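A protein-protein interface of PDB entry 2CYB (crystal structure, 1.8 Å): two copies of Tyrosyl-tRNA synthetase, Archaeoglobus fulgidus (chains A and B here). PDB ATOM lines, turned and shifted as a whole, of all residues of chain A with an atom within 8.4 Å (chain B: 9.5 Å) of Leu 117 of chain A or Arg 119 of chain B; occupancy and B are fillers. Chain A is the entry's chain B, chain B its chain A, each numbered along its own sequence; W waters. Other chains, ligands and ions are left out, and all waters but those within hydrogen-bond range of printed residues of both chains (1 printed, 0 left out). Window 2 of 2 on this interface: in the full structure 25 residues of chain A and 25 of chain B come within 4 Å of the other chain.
Among the printed residues, pairs that only touch across the chains: Ile 73 of chain A with Leu 126 of chain B (3.6 Å), Phe 83 of chain A with Leu 123 of chain B (3.8 Å), Leu 117 of chain A with Arg 119 of chain B (3.7 Å), Leu 117 of chain A with Val 122 of chain B (3.98 Å), Leu 117 of chain A with Leu 126 of chain B (3.9 Å), Arg 119 of chain A with Leu 117 of chain B (3.3 Å), Val 122 of chain A with Leu 117 of chain B (3.7 Å), Val 122 of chain A with Val 122 of chain B (3.6 Å) and Leu 123 of chain A with Leu 117 of chain B (3.7 Å).
Leu 117 of chain A touches just these residues of chain B: Arg 119 (3.7 Å), Val 122 (3.98 Å) and Leu 126 (3.9 Å). Printed residues of chain B within 4 Å of Phe 83 of chain A: Leu 123. Printed residues of chain B within 4 Å of Ile 73 of chain A: Leu 126. Printed residues of chain B within 4 Å of Arg 119 of chain A: Leu 117. His 168 of chain B touches none of the printed residues of chain A. The nearest residue of chain B that does not touch Leu 117 of chain A is Leu 123 of chain B (4.1 Å). The nearest residue of chain A that does not touch Arg 119 of chain B is Ser 113 of chain A (4.6 Å). The nearest printed residue of chain B that does not touch Phe 83 of chain A is Lys 127 of chain B (4.05 Å).
Of the 17 printed residues of chain B, 5 touch a printed residue of chain A. Hydrophobic or aromatic side chains of chain B within 4 Å of the printed part of chain A: Leu 117, Val 122, Leu 123 and Leu 126. Of the 18 printed residues of chain A, 6 touch a printed residue of chain B. Among the printed residues, 9 pairs touch across the chains. Among the printed residues, no Asp or Glu carboxylate lies within 4 Å of a Lys or Arg side-chain nitrogen of the other chain.
Leu 117 of chain A touches Arg 119 of chain B, and with the chains exchanged Arg 119 of chain A touches Leu 117 of chain B. Leu 117 of chain A touches Val 122 of chain B, and with the chains exchanged Val 122 of chain A touches Leu 117 of chain B. Val 122 of chain A touches its own counterpart, Val 122 of chain B. Leu 123 of chain A touches Leu 117 of chain B, but with the chains exchanged Leu 117 of chain A does not touch Leu 123 of chain B (4.1 Å). Positions printed for both chains: 114, 115, 116, 117, 118, 119, 120, 121, 122, 123 and 125.
Water W1 lies within hydrogen-bond range of O of Leu 117 of chain B (2.7 Å), O of Leu 117 of chain A (2.7 Å) and N of Arg 119 of chain B (3.2 Å).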
ATOM      1  N   ASP A  72      -4.069   8.743 -13.770  1.00  0.00           N
ATOM      2  CA  ASP A  72      -2.840   8.021 -14.049  1.00  0.00           C
ATOM      3  C   ASP A  72      -1.734   8.172 -13.008  1.00  0.00           C
ATOM      4  O   ASP A  72      -1.079   7.183 -12.647  1.00  0.00           O
ATOM      5  CB  ASP A  72      -2.322   8.346 -15.470  1.00  0.00           C
ATOM      6  CG  ASP A  72      -2.090   9.839 -15.720  1.00  0.00           C
ATOM      7  OD1 ASP A  72      -1.360  10.145 -16.692  1.00  0.00           O
ATOM      8  OD2 ASP A  72      -2.612  10.711 -14.993  1.00  0.00           O
ATOM      9  N   ILE A  73      -1.527   9.383 -12.500  1.00  0.00           N
ATOM     10  CA  ILE A  73      -0.496   9.582 -11.486  1.00  0.00           C
ATOM     11  C   ILE A  73      -0.892   8.812 -10.216  1.00  0.00           C
ATOM     12  O   ILE A  73      -0.050   8.189  -9.565  1.00  0.00           O
ATOM     13  CB  ILE A  73      -0.310  11.079 -11.147  1.00  0.00           C
ATOM     14  CG1 ILE A  73       0.135  11.859 -12.401  1.00  0.00           C
ATOM     15  CG2 ILE A  73       0.736  11.248 -10.030  1.00  0.00           C
ATOM     16  CD1 ILE A  73       1.386  11.337 -13.051  1.00  0.00           C
ATOM     17  N   PHE A  83       4.888   4.146 -15.651  1.00  0.00           N
ATOM     18  CA  PHE A  83       4.096   5.188 -16.291  1.00  0.00           C
ATOM     19  C   PHE A  83       3.672   4.727 -17.685  1.00  0.00           C
ATOM     20  O   PHE A  83       2.556   4.993 -18.135  1.00  0.00           O
ATOM     21  CB  PHE A  83       4.893   6.487 -16.397  1.00  0.00           C
ATOM     22  CG  PHE A  83       4.990   7.250 -15.102  1.00  0.00           C
ATOM     23  CD1 PHE A  83       6.185   7.299 -14.389  1.00  0.00           C
ATOM     24  CD2 PHE A  83       3.881   7.920 -14.595  1.00  0.00           C
ATOM     25  CE1 PHE A  83       6.276   8.009 -13.187  1.00  0.00           C
ATOM     26  CE2 PHE A  83       3.959   8.631 -13.393  1.00  0.00           C
ATOM     27  CZ  PHE A  83       5.160   8.675 -12.690  1.00  0.00           C
ATOM     28  N   LEU A 111      -7.001  13.681 -18.061  1.00  0.00           N
ATOM     29  CA  LEU A 111      -5.943  12.771 -17.642  1.00  0.00           C
ATOM     30  C   LEU A 111      -5.208  13.492 -16.508  1.00  0.00           C
ATOM     31  O   LEU A 111      -4.814  14.653 -16.651  1.00  0.00           O
ATOM     32  CB  LEU A 111      -4.987  12.474 -18.810  1.00  0.00           C
ATOM     33  CG  LEU A 111      -3.883  11.450 -18.519  1.00  0.00           C
ATOM     34  CD1 LEU A 111      -4.490  10.075 -18.229  1.00  0.00           C
ATOM     35  CD2 LEU A 111      -2.949  11.353 -19.738  1.00  0.00           C
ATOM     36  N   GLY A 112      -5.041  12.821 -15.370  1.00  0.00           N
ATOM     37  CA  GLY A 112      -4.394  13.462 -14.234  1.00  0.00           C
ATOM     38  C   GLY A 112      -3.087  14.192 -14.522  1.00  0.00           C
ATOM     39  O   GLY A 112      -2.899  15.354 -14.130  1.00  0.00           O
ATOM     40  N   SER A 113      -2.191  13.512 -15.220  1.00  0.00           N
ATOM     41  CA  SER A 113      -0.884  14.072 -15.534  1.00  0.00           C
ATOM     42  C   SER A 113      -0.945  15.365 -16.350  1.00  0.00           C
ATOM     43  O   SER A 113       0.071  16.045 -16.498  1.00  0.00           O
ATOM     44  CB  SER A 113      -0.030  13.024 -16.254  1.00  0.00           C
ATOM     45  OG  SER A 113      -0.647  12.578 -17.454  1.00  0.00           O
ATOM     46  N   GLU A 114      -2.126  15.709 -16.861  1.00  0.00           N
ATOM     47  CA  GLU A 114      -2.292  16.943 -17.634  1.00  0.00           C
ATOM     48  C   GLU A 114      -2.128  18.167 -16.739  1.00  0.00           C
ATOM     49  O   GLU A 114      -1.738  19.235 -17.209  1.00  0.00           O
ATOM     50  CB  GLU A 114      -3.685  17.038 -18.267  1.00  0.00           C
ATOM     51  CG  GLU A 114      -4.069  15.959 -19.255  1.00  0.00           C
ATOM     52  CD  GLU A 114      -5.523  16.100 -19.720  1.00  0.00           C
ATOM     53  OE1 GLU A 114      -6.043  15.163 -20.352  1.00  0.00           O
ATOM     54  OE2 GLU A 114      -6.143  17.152 -19.458  1.00  0.00           O
ATOM     55  N   TYR A 115      -2.448  18.031 -15.455  1.00  0.00           N
ATOM     56  CA  TYR A 115      -2.335  19.168 -14.557  1.00  0.00           C
ATOM     57  C   TYR A 115      -1.707  18.869 -13.196  1.00  0.00           C
ATOM     58  O   TYR A 115      -1.335  19.788 -12.471  1.00  0.00           O
ATOM     59  CB  TYR A 115      -3.716  19.800 -14.321  1.00  0.00           C
ATOM     60  CG  TYR A 115      -4.671  18.910 -13.532  1.00  0.00           C
ATOM     61  CD1 TYR A 115      -5.435  17.935 -14.173  1.00  0.00           C
ATOM     62  CD2 TYR A 115      -4.755  19.004 -12.140  1.00  0.00           C
ATOM     63  CE1 TYR A 115      -6.263  17.066 -13.446  1.00  0.00           C
ATOM     64  CE2 TYR A 115      -5.575  18.136 -11.403  1.00  0.00           C
ATOM     65  CZ  TYR A 115      -6.321  17.173 -12.065  1.00  0.00           C
ATOM     66  OH  TYR A 115      -7.108  16.289 -11.351  1.00  0.00           O
ATOM     67  N   GLN A 116      -1.573  17.595 -12.840  1.00  0.00           N
ATOM     68  CA  GLN A 116      -1.051  17.270 -11.514  1.00  0.00           C
ATOM     69  C   GLN A 116       0.441  17.486 -11.298  1.00  0.00           C
ATOM     70  O   GLN A 116       0.948  17.273 -10.194  1.00  0.00           O
ATOM     71  CB  GLN A 116      -1.452  15.838 -11.146  1.00  0.00           C
ATOM     72  CG  GLN A 116      -2.967  15.696 -10.983  1.00  0.00           C
ATOM     73  CD  GLN A 116      -3.400  14.252 -10.868  1.00  0.00           C
ATOM     74  OE1 GLN A 116      -2.792  13.361 -11.475  1.00  0.00           O
ATOM     75  NE2 GLN A 116      -4.480  14.009 -10.130  1.00  0.00           N
ATOM     76  N   LEU A 117       1.144  17.899 -12.348  1.00  0.00           N
ATOM     77  CA  LEU A 117       2.562  18.175 -12.235  1.00  0.00           C
ATOM     78  C   LEU A 117       2.824  19.666 -12.440  1.00  0.00           C
ATOM     79  O   LEU A 117       3.974  20.091 -12.486  1.00  0.00           O
ATOM     80  CB  LEU A 117       3.349  17.353 -13.258  1.00  0.00           C
ATOM     81  CG  LEU A 117       3.241  15.833 -13.133  1.00  0.00           C
ATOM     82  CD1 LEU A 117       3.848  15.176 -14.367  1.00  0.00           C
ATOM     83  CD2 LEU A 117       3.944  15.371 -11.871  1.00  0.00           C
ATOM     84  N   SER A 118       1.761  20.463 -12.552  1.00  0.00           N
ATOM     85  CA  SER A 118       1.912  21.904 -12.743  1.00  0.00           C
ATOM     86  C   SER A 118       2.277  22.599 -11.433  1.00  0.00           C
ATOM     87  O   SER A 118       1.971  22.104 -10.346  1.00  0.00           O
ATOM     88  CB  SER A 118       0.626  22.513 -13.316  1.00  0.00           C
ATOM     89  OG  SER A 118      -0.440  22.433 -12.387  1.00  0.00           O
ATOM     90  N   ARG A 119       2.926  23.756 -11.543  1.00  0.00           N
ATOM     91  CA  ARG A 119       3.366  24.514 -10.368  1.00  0.00           C
ATOM     92  C   ARG A 119       2.287  24.825  -9.325  1.00  0.00           C
ATOM     93  O   ARG A 119       2.494  24.603  -8.132  1.00  0.00           O
ATOM     94  CB  ARG A 119       4.021  25.829 -10.807  1.00  0.00           C
ATOM     95  CG  ARG A 119       4.530  26.670  -9.641  1.00  0.00           C
ATOM     96  CD  ARG A 119       4.560  28.155  -9.978  1.00  0.00           C
ATOM     97  NE  ARG A 119       5.000  28.958  -8.840  1.00  0.00           N
ATOM     98  CZ  ARG A 119       6.232  28.931  -8.339  1.00  0.00           C
ATOM     99  NH1 ARG A 119       6.546  29.692  -7.299  1.00  0.00           N
ATOM    100  NH2 ARG A 119       7.154  28.150  -8.888  1.00  0.00           N
ATOM    101  N   ASP A 120       1.154  25.362  -9.764  1.00  0.00           N
ATOM    102  CA  ASP A 120       0.075  25.713  -8.849  1.00  0.00           C
ATOM    103  C   ASP A 120      -0.472  24.505  -8.104  1.00  0.00           C
ATOM    104  O   ASP A 120      -0.788  24.583  -6.914  1.00  0.00           O
ATOM    105  CB  ASP A 120      -1.062  26.376  -9.609  1.00  0.00           C
ATOM    106  CG  ASP A 120      -0.700  27.760 -10.086  1.00  0.00           C
ATOM    107  OD1 ASP A 120      -1.546  28.396 -10.750  1.00  0.00           O
ATOM    108  OD2 ASP A 120       0.431  28.205  -9.787  1.00  0.00           O
ATOM    109  N   TYR A 121      -0.613  23.404  -8.823  1.00  0.00           N
ATOM    110  CA  TYR A 121      -1.128  22.175  -8.217  1.00  0.00           C
ATOM    111  C   TYR A 121      -0.120  21.619  -7.222  1.00  0.00           C
ATOM    112  O   TYR A 121      -0.477  21.278  -6.097  1.00  0.00           O
ATOM    113  CB  TYR A 121      -1.408  21.131  -9.290  1.00  0.00           C
ATOM    114  CG  TYR A 121      -2.029  19.860  -8.745  1.00  0.00           C
ATOM    115  CD1 TYR A 121      -3.415  19.731  -8.612  1.00  0.00           C
ATOM    116  CD2 TYR A 121      -1.223  18.784  -8.378  1.00  0.00           C
ATOM    117  CE1 TYR A 121      -3.992  18.531  -8.125  1.00  0.00           C
ATOM    118  CE2 TYR A 121      -1.773  17.600  -7.896  1.00  0.00           C
ATOM    119  CZ  TYR A 121      -3.148  17.477  -7.777  1.00  0.00           C
ATOM    120  OH  TYR A 121      -3.673  16.277  -7.336  1.00  0.00           O
ATOM    121  N   VAL A 122       1.139  21.529  -7.640  1.00  0.00           N
ATOM    122  CA  VAL A 122       2.192  21.008  -6.772  1.00  0.00           C
ATOM    123  C   VAL A 122       2.339  21.850  -5.504  1.00  0.00           C
ATOM    124  O   VAL A 122       2.560  21.311  -4.419  1.00  0.00           O
ATOM    125  CB  VAL A 122       3.537  20.922  -7.526  1.00  0.00           C
ATOM    126  CG1 VAL A 122       4.668  20.672  -6.540  1.00  0.00           C
ATOM    127  CG2 VAL A 122       3.475  19.767  -8.564  1.00  0.00           C
ATOM    128  N   LEU A 123       2.208  23.166  -5.625  1.00  0.00           N
ATOM    129  CA  LEU A 123       2.295  24.019  -4.442  1.00  0.00           C
ATOM    130  C   LEU A 123       1.147  23.684  -3.479  1.00  0.00           C
ATOM    131  O   LEU A 123       1.340  23.650  -2.258  1.00  0.00           O
ATOM    132  CB  LEU A 123       2.218  25.501  -4.825  1.00  0.00           C
ATOM    133  CG  LEU A 123       3.475  26.340  -4.591  1.00  0.00           C
ATOM    134  CD1 LEU A 123       3.167  27.795  -4.915  1.00  0.00           C
ATOM    135  CD2 LEU A 123       3.937  26.207  -3.148  1.00  0.00           C
ATOM    136  N   VAL A 125      -0.283  20.833  -3.187  1.00  0.00           N
ATOM    137  CA  VAL A 125      -0.002  19.532  -2.578  1.00  0.00           C
ATOM    138  C   VAL A 125       0.878  19.747  -1.334  1.00  0.00           C
ATOM    139  O   VAL A 125       0.655  19.123  -0.286  1.00  0.00           O
ATOM    140  CB  VAL A 125       0.706  18.577  -3.577  1.00  0.00           C
ATOM    141  CG1 VAL A 125       1.201  17.336  -2.854  1.00  0.00           C
ATOM    142  CG2 VAL A 125      -0.261  18.163  -4.693  1.00  0.00           C
ATOM    143  N   MET A 161      -3.657  14.526  -3.034  1.00  0.00           N
ATOM    144  CA  MET A 161      -3.892  14.852  -4.439  1.00  0.00           C
ATOM    145  C   MET A 161      -5.337  14.622  -4.850  1.00  0.00           C
ATOM    146  O   MET A 161      -5.881  15.401  -5.625  1.00  0.00           O
ATOM    147  CB  MET A 161      -2.943  14.058  -5.340  1.00  0.00           C
ATOM    148  CG  MET A 161      -1.511  14.576  -5.304  1.00  0.00           C
ATOM    149  SD  MET A 161      -0.417  13.556  -6.301  1.00  0.00           S
ATOM    150  CE  MET A 161      -1.234  13.627  -7.871  1.00  0.00           C
ATOM    151  N   GLU B 114      13.524  27.779  -6.372  1.00  0.00           N
ATOM    152  CA  GLU B 114      14.010  28.057  -7.730  1.00  0.00           C
ATOM    153  C   GLU B 114      13.866  26.870  -8.685  1.00  0.00           C
ATOM    154  O   GLU B 114      13.745  27.051  -9.902  1.00  0.00           O
ATOM    155  CB  GLU B 114      15.491  28.448  -7.705  1.00  0.00           C
ATOM    156  CG  GLU B 114      15.810  29.850  -7.239  1.00  0.00           C
ATOM    157  CD  GLU B 114      17.313  30.128  -7.278  1.00  0.00           C
ATOM    158  OE1 GLU B 114      17.966  29.719  -8.262  1.00  0.00           O
ATOM    159  OE2 GLU B 114      17.840  30.753  -6.333  1.00  0.00           O
ATOM    160  N   TYR B 115      13.896  25.657  -8.141  1.00  0.00           N
ATOM    161  CA  TYR B 115      13.796  24.466  -8.970  1.00  0.00           C
ATOM    162  C   TYR B 115      12.947  23.338  -8.379  1.00  0.00           C
ATOM    163  O   TYR B 115      12.597  22.401  -9.089  1.00  0.00           O
ATOM    164  CB  TYR B 115      15.194  23.910  -9.237  1.00  0.00           C
ATOM    165  CG  TYR B 115      15.873  23.416  -7.975  1.00  0.00           C
ATOM    166  CD1 TYR B 115      16.558  24.297  -7.136  1.00  0.00           C
ATOM    167  CD2 TYR B 115      15.794  22.072  -7.599  1.00  0.00           C
ATOM    168  CE1 TYR B 115      17.159  23.852  -5.949  1.00  0.00           C
ATOM    169  CE2 TYR B 115      16.384  21.615  -6.413  1.00  0.00           C
ATOM    170  CZ  TYR B 115      17.065  22.510  -5.595  1.00  0.00           C
ATOM    171  OH  TYR B 115      17.657  22.062  -4.426  1.00  0.00           O
ATOM    172  N   GLN B 116      12.625  23.411  -7.091  1.00  0.00           N
ATOM    173  CA  GLN B 116      11.854  22.333  -6.462  1.00  0.00           C
ATOM    174  C   GLN B 116      10.382  22.225  -6.864  1.00  0.00           C
ATOM    175  O   GLN B 116       9.685  21.320  -6.409  1.00  0.00           O
ATOM    176  CB  GLN B 116      11.981  22.422  -4.937  1.00  0.00           C
ATOM    177  CG  GLN B 116      13.409  22.227  -4.479  1.00  0.00           C
ATOM    178  CD  GLN B 116      13.612  22.497  -2.996  1.00  0.00           C
ATOM    179  OE1 GLN B 116      12.943  23.342  -2.400  1.00  0.00           O
ATOM    180  NE2 GLN B 116      14.559  21.791  -2.402  1.00  0.00           N
ATOM    181  N   LEU B 117       9.904  23.140  -7.706  1.00  0.00           N
ATOM    182  CA  LEU B 117       8.518  23.081  -8.167  1.00  0.00           C
ATOM    183  C   LEU B 117       8.488  22.809  -9.664  1.00  0.00           C
ATOM    184  O   LEU B 117       7.419  22.793 -10.281  1.00  0.00           O
ATOM    185  CB  LEU B 117       7.781  24.389  -7.870  1.00  0.00           C
ATOM    186  CG  LEU B 117       7.532  24.749  -6.402  1.00  0.00           C
ATOM    187  CD1 LEU B 117       6.787  26.075  -6.324  1.00  0.00           C
ATOM    188  CD2 LEU B 117       6.720  23.646  -5.728  1.00  0.00           C
ATOM    189  N   SER B 118       9.662  22.594 -10.247  1.00  0.00           N
ATOM    190  CA  SER B 118       9.763  22.321 -11.681  1.00  0.00           C
ATOM    191  C   SER B 118       9.225  20.924 -11.990  1.00  0.00           C
ATOM    192  O   SER B 118       9.273  20.035 -11.145  1.00  0.00           O
ATOM    193  CB  SER B 118      11.218  22.444 -12.148  1.00  0.00           C
ATOM    194  OG  SER B 118      12.002  21.350 -11.714  1.00  0.00           O
ATOM    195  N   ARG B 119       8.720  20.732 -13.207  1.00  0.00           N
ATOM    196  CA  ARG B 119       8.146  19.449 -13.600  1.00  0.00           C
ATOM    197  C   ARG B 119       9.085  18.260 -13.426  1.00  0.00           C
ATOM    198  O   ARG B 119       8.669  17.201 -12.949  1.00  0.00           O
ATOM    199  CB  ARG B 119       7.680  19.495 -15.054  1.00  0.00           C
ATOM    200  CG  ARG B 119       7.056  18.187 -15.521  1.00  0.00           C
ATOM    201  CD  ARG B 119       7.193  18.004 -17.020  1.00  0.00           C
ATOM    202  NE  ARG B 119       6.574  16.761 -17.466  1.00  0.00           N
ATOM    203  CZ  ARG B 119       5.262  16.558 -17.512  1.00  0.00           C
ATOM    204  NH1 ARG B 119       4.782  15.394 -17.929  1.00  0.00           N
ATOM    205  NH2 ARG B 119       4.429  17.527 -17.153  1.00  0.00           N
ATOM    206  N   ASP B 120      10.342  18.418 -13.828  1.00  0.00           N
ATOM    207  CA  ASP B 120      11.297  17.323 -13.696  1.00  0.00           C
ATOM    208  C   ASP B 120      11.575  16.978 -12.238  1.00  0.00           C
ATOM    209  O   ASP B 120      11.731  15.807 -11.885  1.00  0.00           O
ATOM    210  CB  ASP B 120      12.617  17.662 -14.391  1.00  0.00           C
ATOM    211  CG  ASP B 120      12.581  17.374 -15.878  1.00  0.00           C
ATOM    212  OD1 ASP B 120      13.618  17.565 -16.546  1.00  0.00           O
ATOM    213  OD2 ASP B 120      11.517  16.950 -16.376  1.00  0.00           O
ATOM    214  N   TYR B 121      11.639  17.995 -11.392  1.00  0.00           N
ATOM    215  CA  TYR B 121      11.906  17.750  -9.977  1.00  0.00           C
ATOM    216  C   TYR B 121      10.707  17.098  -9.287  1.00  0.00           C
ATOM    217  O   TYR B 121      10.866  16.146  -8.523  1.00  0.00           O
ATOM    218  CB  TYR B 121      12.245  19.049  -9.262  1.00  0.00           C
ATOM    219  CG  TYR B 121      12.656  18.846  -7.819  1.00  0.00           C
ATOM    220  CD1 TYR B 121      13.993  18.638  -7.471  1.00  0.00           C
ATOM    221  CD2 TYR B 121      11.704  18.881  -6.801  1.00  0.00           C
ATOM    222  CE1 TYR B 121      14.374  18.482  -6.129  1.00  0.00           C
ATOM    223  CE2 TYR B 121      12.073  18.719  -5.457  1.00  0.00           C
ATOM    224  CZ  TYR B 121      13.402  18.526  -5.130  1.00  0.00           C
ATOM    225  OH  TYR B 121      13.751  18.418  -3.799  1.00  0.00           O
ATOM    226  N   VAL B 122       9.507  17.596  -9.554  1.00  0.00           N
ATOM    227  CA  VAL B 122       8.326  17.012  -8.922  1.00  0.00           C
ATOM    228  C   VAL B 122       8.130  15.565  -9.358  1.00  0.00           C
ATOM    229  O   VAL B 122       7.764  14.708  -8.556  1.00  0.00           O
ATOM    230  CB  VAL B 122       7.051  17.828  -9.228  1.00  0.00           C
ATOM    231  CG1 VAL B 122       7.188  19.224  -8.654  1.00  0.00           C
ATOM    232  CG2 VAL B 122       6.804  17.887 -10.719  1.00  0.00           C
ATOM    233  N   LEU B 123       8.394  15.277 -10.626  1.00  0.00           N
ATOM    234  CA  LEU B 123       8.243  13.915 -11.097  1.00  0.00           C
ATOM    235  C   LEU B 123       9.222  13.009 -10.345  1.00  0.00           C
ATOM    236  O   LEU B 123       8.877  11.876  -9.984  1.00  0.00           O
ATOM    237  CB  LEU B 123       8.480  13.857 -12.608  1.00  0.00           C
ATOM    238  CG  LEU B 123       7.795  12.763 -13.432  1.00  0.00           C
ATOM    239  CD1 LEU B 123       6.506  12.273 -12.779  1.00  0.00           C
ATOM    240  CD2 LEU B 123       7.495  13.351 -14.805  1.00  0.00           C
ATOM    241  N   ASP B 124      10.435  13.504 -10.090  1.00  0.00           N
ATOM    242  CA  ASP B 124      11.419  12.711  -9.351  1.00  0.00           C
ATOM    243  C   ASP B 124      10.937  12.454  -7.924  1.00  0.00           C
ATOM    244  O   ASP B 124      11.172  11.377  -7.364  1.00  0.00           O
ATOM    245  CB  ASP B 124      12.771  13.423  -9.307  1.00  0.00           C
ATOM    246  CG  ASP B 124      13.617  13.141 -10.532  1.00  0.00           C
ATOM    247  OD1 ASP B 124      14.603  13.871 -10.741  1.00  0.00           O
ATOM    248  OD2 ASP B 124      13.298  12.188 -11.275  1.00  0.00           O
ATOM    249  N   VAL B 125      10.286  13.452  -7.335  1.00  0.00           N
ATOM    250  CA  VAL B 125       9.760  13.314  -5.979  1.00  0.00           C
ATOM    251  C   VAL B 125       8.745  12.184  -5.966  1.00  0.00           C
ATOM    252  O   VAL B 125       8.754  11.336  -5.068  1.00  0.00           O
ATOM    253  CB  VAL B 125       9.074  14.620  -5.487  1.00  0.00           C
ATOM    254  CG1 VAL B 125       8.308  14.353  -4.190  1.00  0.00           C
ATOM    255  CG2 VAL B 125      10.116  15.696  -5.258  1.00  0.00           C
ATOM    256  N   LEU B 126       7.872  12.161  -6.972  1.00  0.00           N
ATOM    257  CA  LEU B 126       6.861  11.112  -7.042  1.00  0.00           C
ATOM    258  C   LEU B 126       7.497   9.730  -7.202  1.00  0.00           C
ATOM    259  O   LEU B 126       7.032   8.755  -6.608  1.00  0.00           O
ATOM    260  CB  LEU B 126       5.881  11.389  -8.188  1.00  0.00           C
ATOM    261  CG  LEU B 126       5.020  12.648  -8.040  1.00  0.00           C
ATOM    262  CD1 LEU B 126       3.931  12.618  -9.091  1.00  0.00           C
ATOM    263  CD2 LEU B 126       4.409  12.731  -6.643  1.00  0.00           C
ATOM    264  N   LYS B 127       8.559   9.648  -7.997  1.00  0.00           N
ATOM    265  CA  LYS B 127       9.262   8.384  -8.209  1.00  0.00           C
ATOM    266  C   LYS B 127       9.940   7.958  -6.910  1.00  0.00           C
ATOM    267  O   LYS B 127       9.886   6.784  -6.520  1.00  0.00           O
ATOM    268  CB  LYS B 127      10.305   8.539  -9.316  1.00  0.00           C
ATOM    269  CG  LYS B 127       9.700   8.751 -10.696  1.00  0.00           C
ATOM    270  CD  LYS B 127      10.780   8.979 -11.750  1.00  0.00           C
ATOM    271  CE  LYS B 127      10.174   9.099 -13.142  1.00  0.00           C
ATOM    272  NZ  LYS B 127      11.216   9.308 -14.188  1.00  0.00           N
ATOM    273  N   LEU B 164      16.840  14.403  -3.317  1.00  0.00           N
ATOM    274  CA  LEU B 164      16.804  14.885  -4.694  1.00  0.00           C
ATOM    275  C   LEU B 164      17.571  16.180  -4.902  1.00  0.00           C
ATOM    276  O   LEU B 164      18.025  16.457  -6.017  1.00  0.00           O
ATOM    277  CB  LEU B 164      15.364  15.060  -5.171  1.00  0.00           C
ATOM    278  CG  LEU B 164      14.667  13.740  -5.507  1.00  0.00           C
ATOM    279  CD1 LEU B 164      13.174  13.992  -5.751  1.00  0.00           C
ATOM    280  CD2 LEU B 164      15.340  13.110  -6.740  1.00  0.00           C
ATOM    281  N   HIS B 168      19.798  17.139  -8.198  1.00  0.00           N
ATOM    282  CA  HIS B 168      19.455  18.305  -9.000  1.00  0.00           C
ATOM    283  C   HIS B 168      20.427  19.477  -8.912  1.00  0.00           C
ATOM    284  O   HIS B 168      20.448  20.324  -9.804  1.00  0.00           O
ATOM    285  CB  HIS B 168      18.025  18.748  -8.684  1.00  0.00           C
ATOM    286  CG  HIS B 168      16.984  17.852  -9.282  1.00  0.00           C
ATOM    287  ND1 HIS B 168      16.231  18.213 -10.376  1.00  0.00           N
ATOM    288  CD2 HIS B 168      16.618  16.585  -8.973  1.00  0.00           C
ATOM    289  CE1 HIS B 168      15.444  17.207 -10.719  1.00  0.00           C
ATOM    290  NE2 HIS B 168      15.660  16.206  -9.884  1.00  0.00           N
ATOM    291  N   TYR B 196      20.645   8.663 -10.935  1.00  0.00           N
ATOM    292  CA  TYR B 196      21.609   9.630 -10.420  1.00  0.00           C
ATOM    293  C   TYR B 196      22.698   8.920  -9.625  1.00  0.00           C
ATOM    294  O   TYR B 196      22.498   7.812  -9.143  1.00  0.00           O
ATOM    295  CB  TYR B 196      20.915  10.660  -9.528  1.00  0.00           C
ATOM    296  CG  TYR B 196      19.810  11.419 -10.223  1.00  0.00           C
ATOM    297  CD1 TYR B 196      18.483  11.276  -9.820  1.00  0.00           C
ATOM    298  CD2 TYR B 196      20.090  12.293 -11.271  1.00  0.00           C
ATOM    299  CE1 TYR B 196      17.461  11.988 -10.438  1.00  0.00           C
ATOM    300  CE2 TYR B 196      19.072  13.012 -11.903  1.00  0.00           C
ATOM    301  CZ  TYR B 196      17.761  12.852 -11.477  1.00  0.00           C
ATOM    302  OH  TYR B 196      16.753  13.562 -12.081  1.00  0.00           O
HETATM  303  O   HOH W   1       5.912  21.916 -12.297  1.00  0.00           O
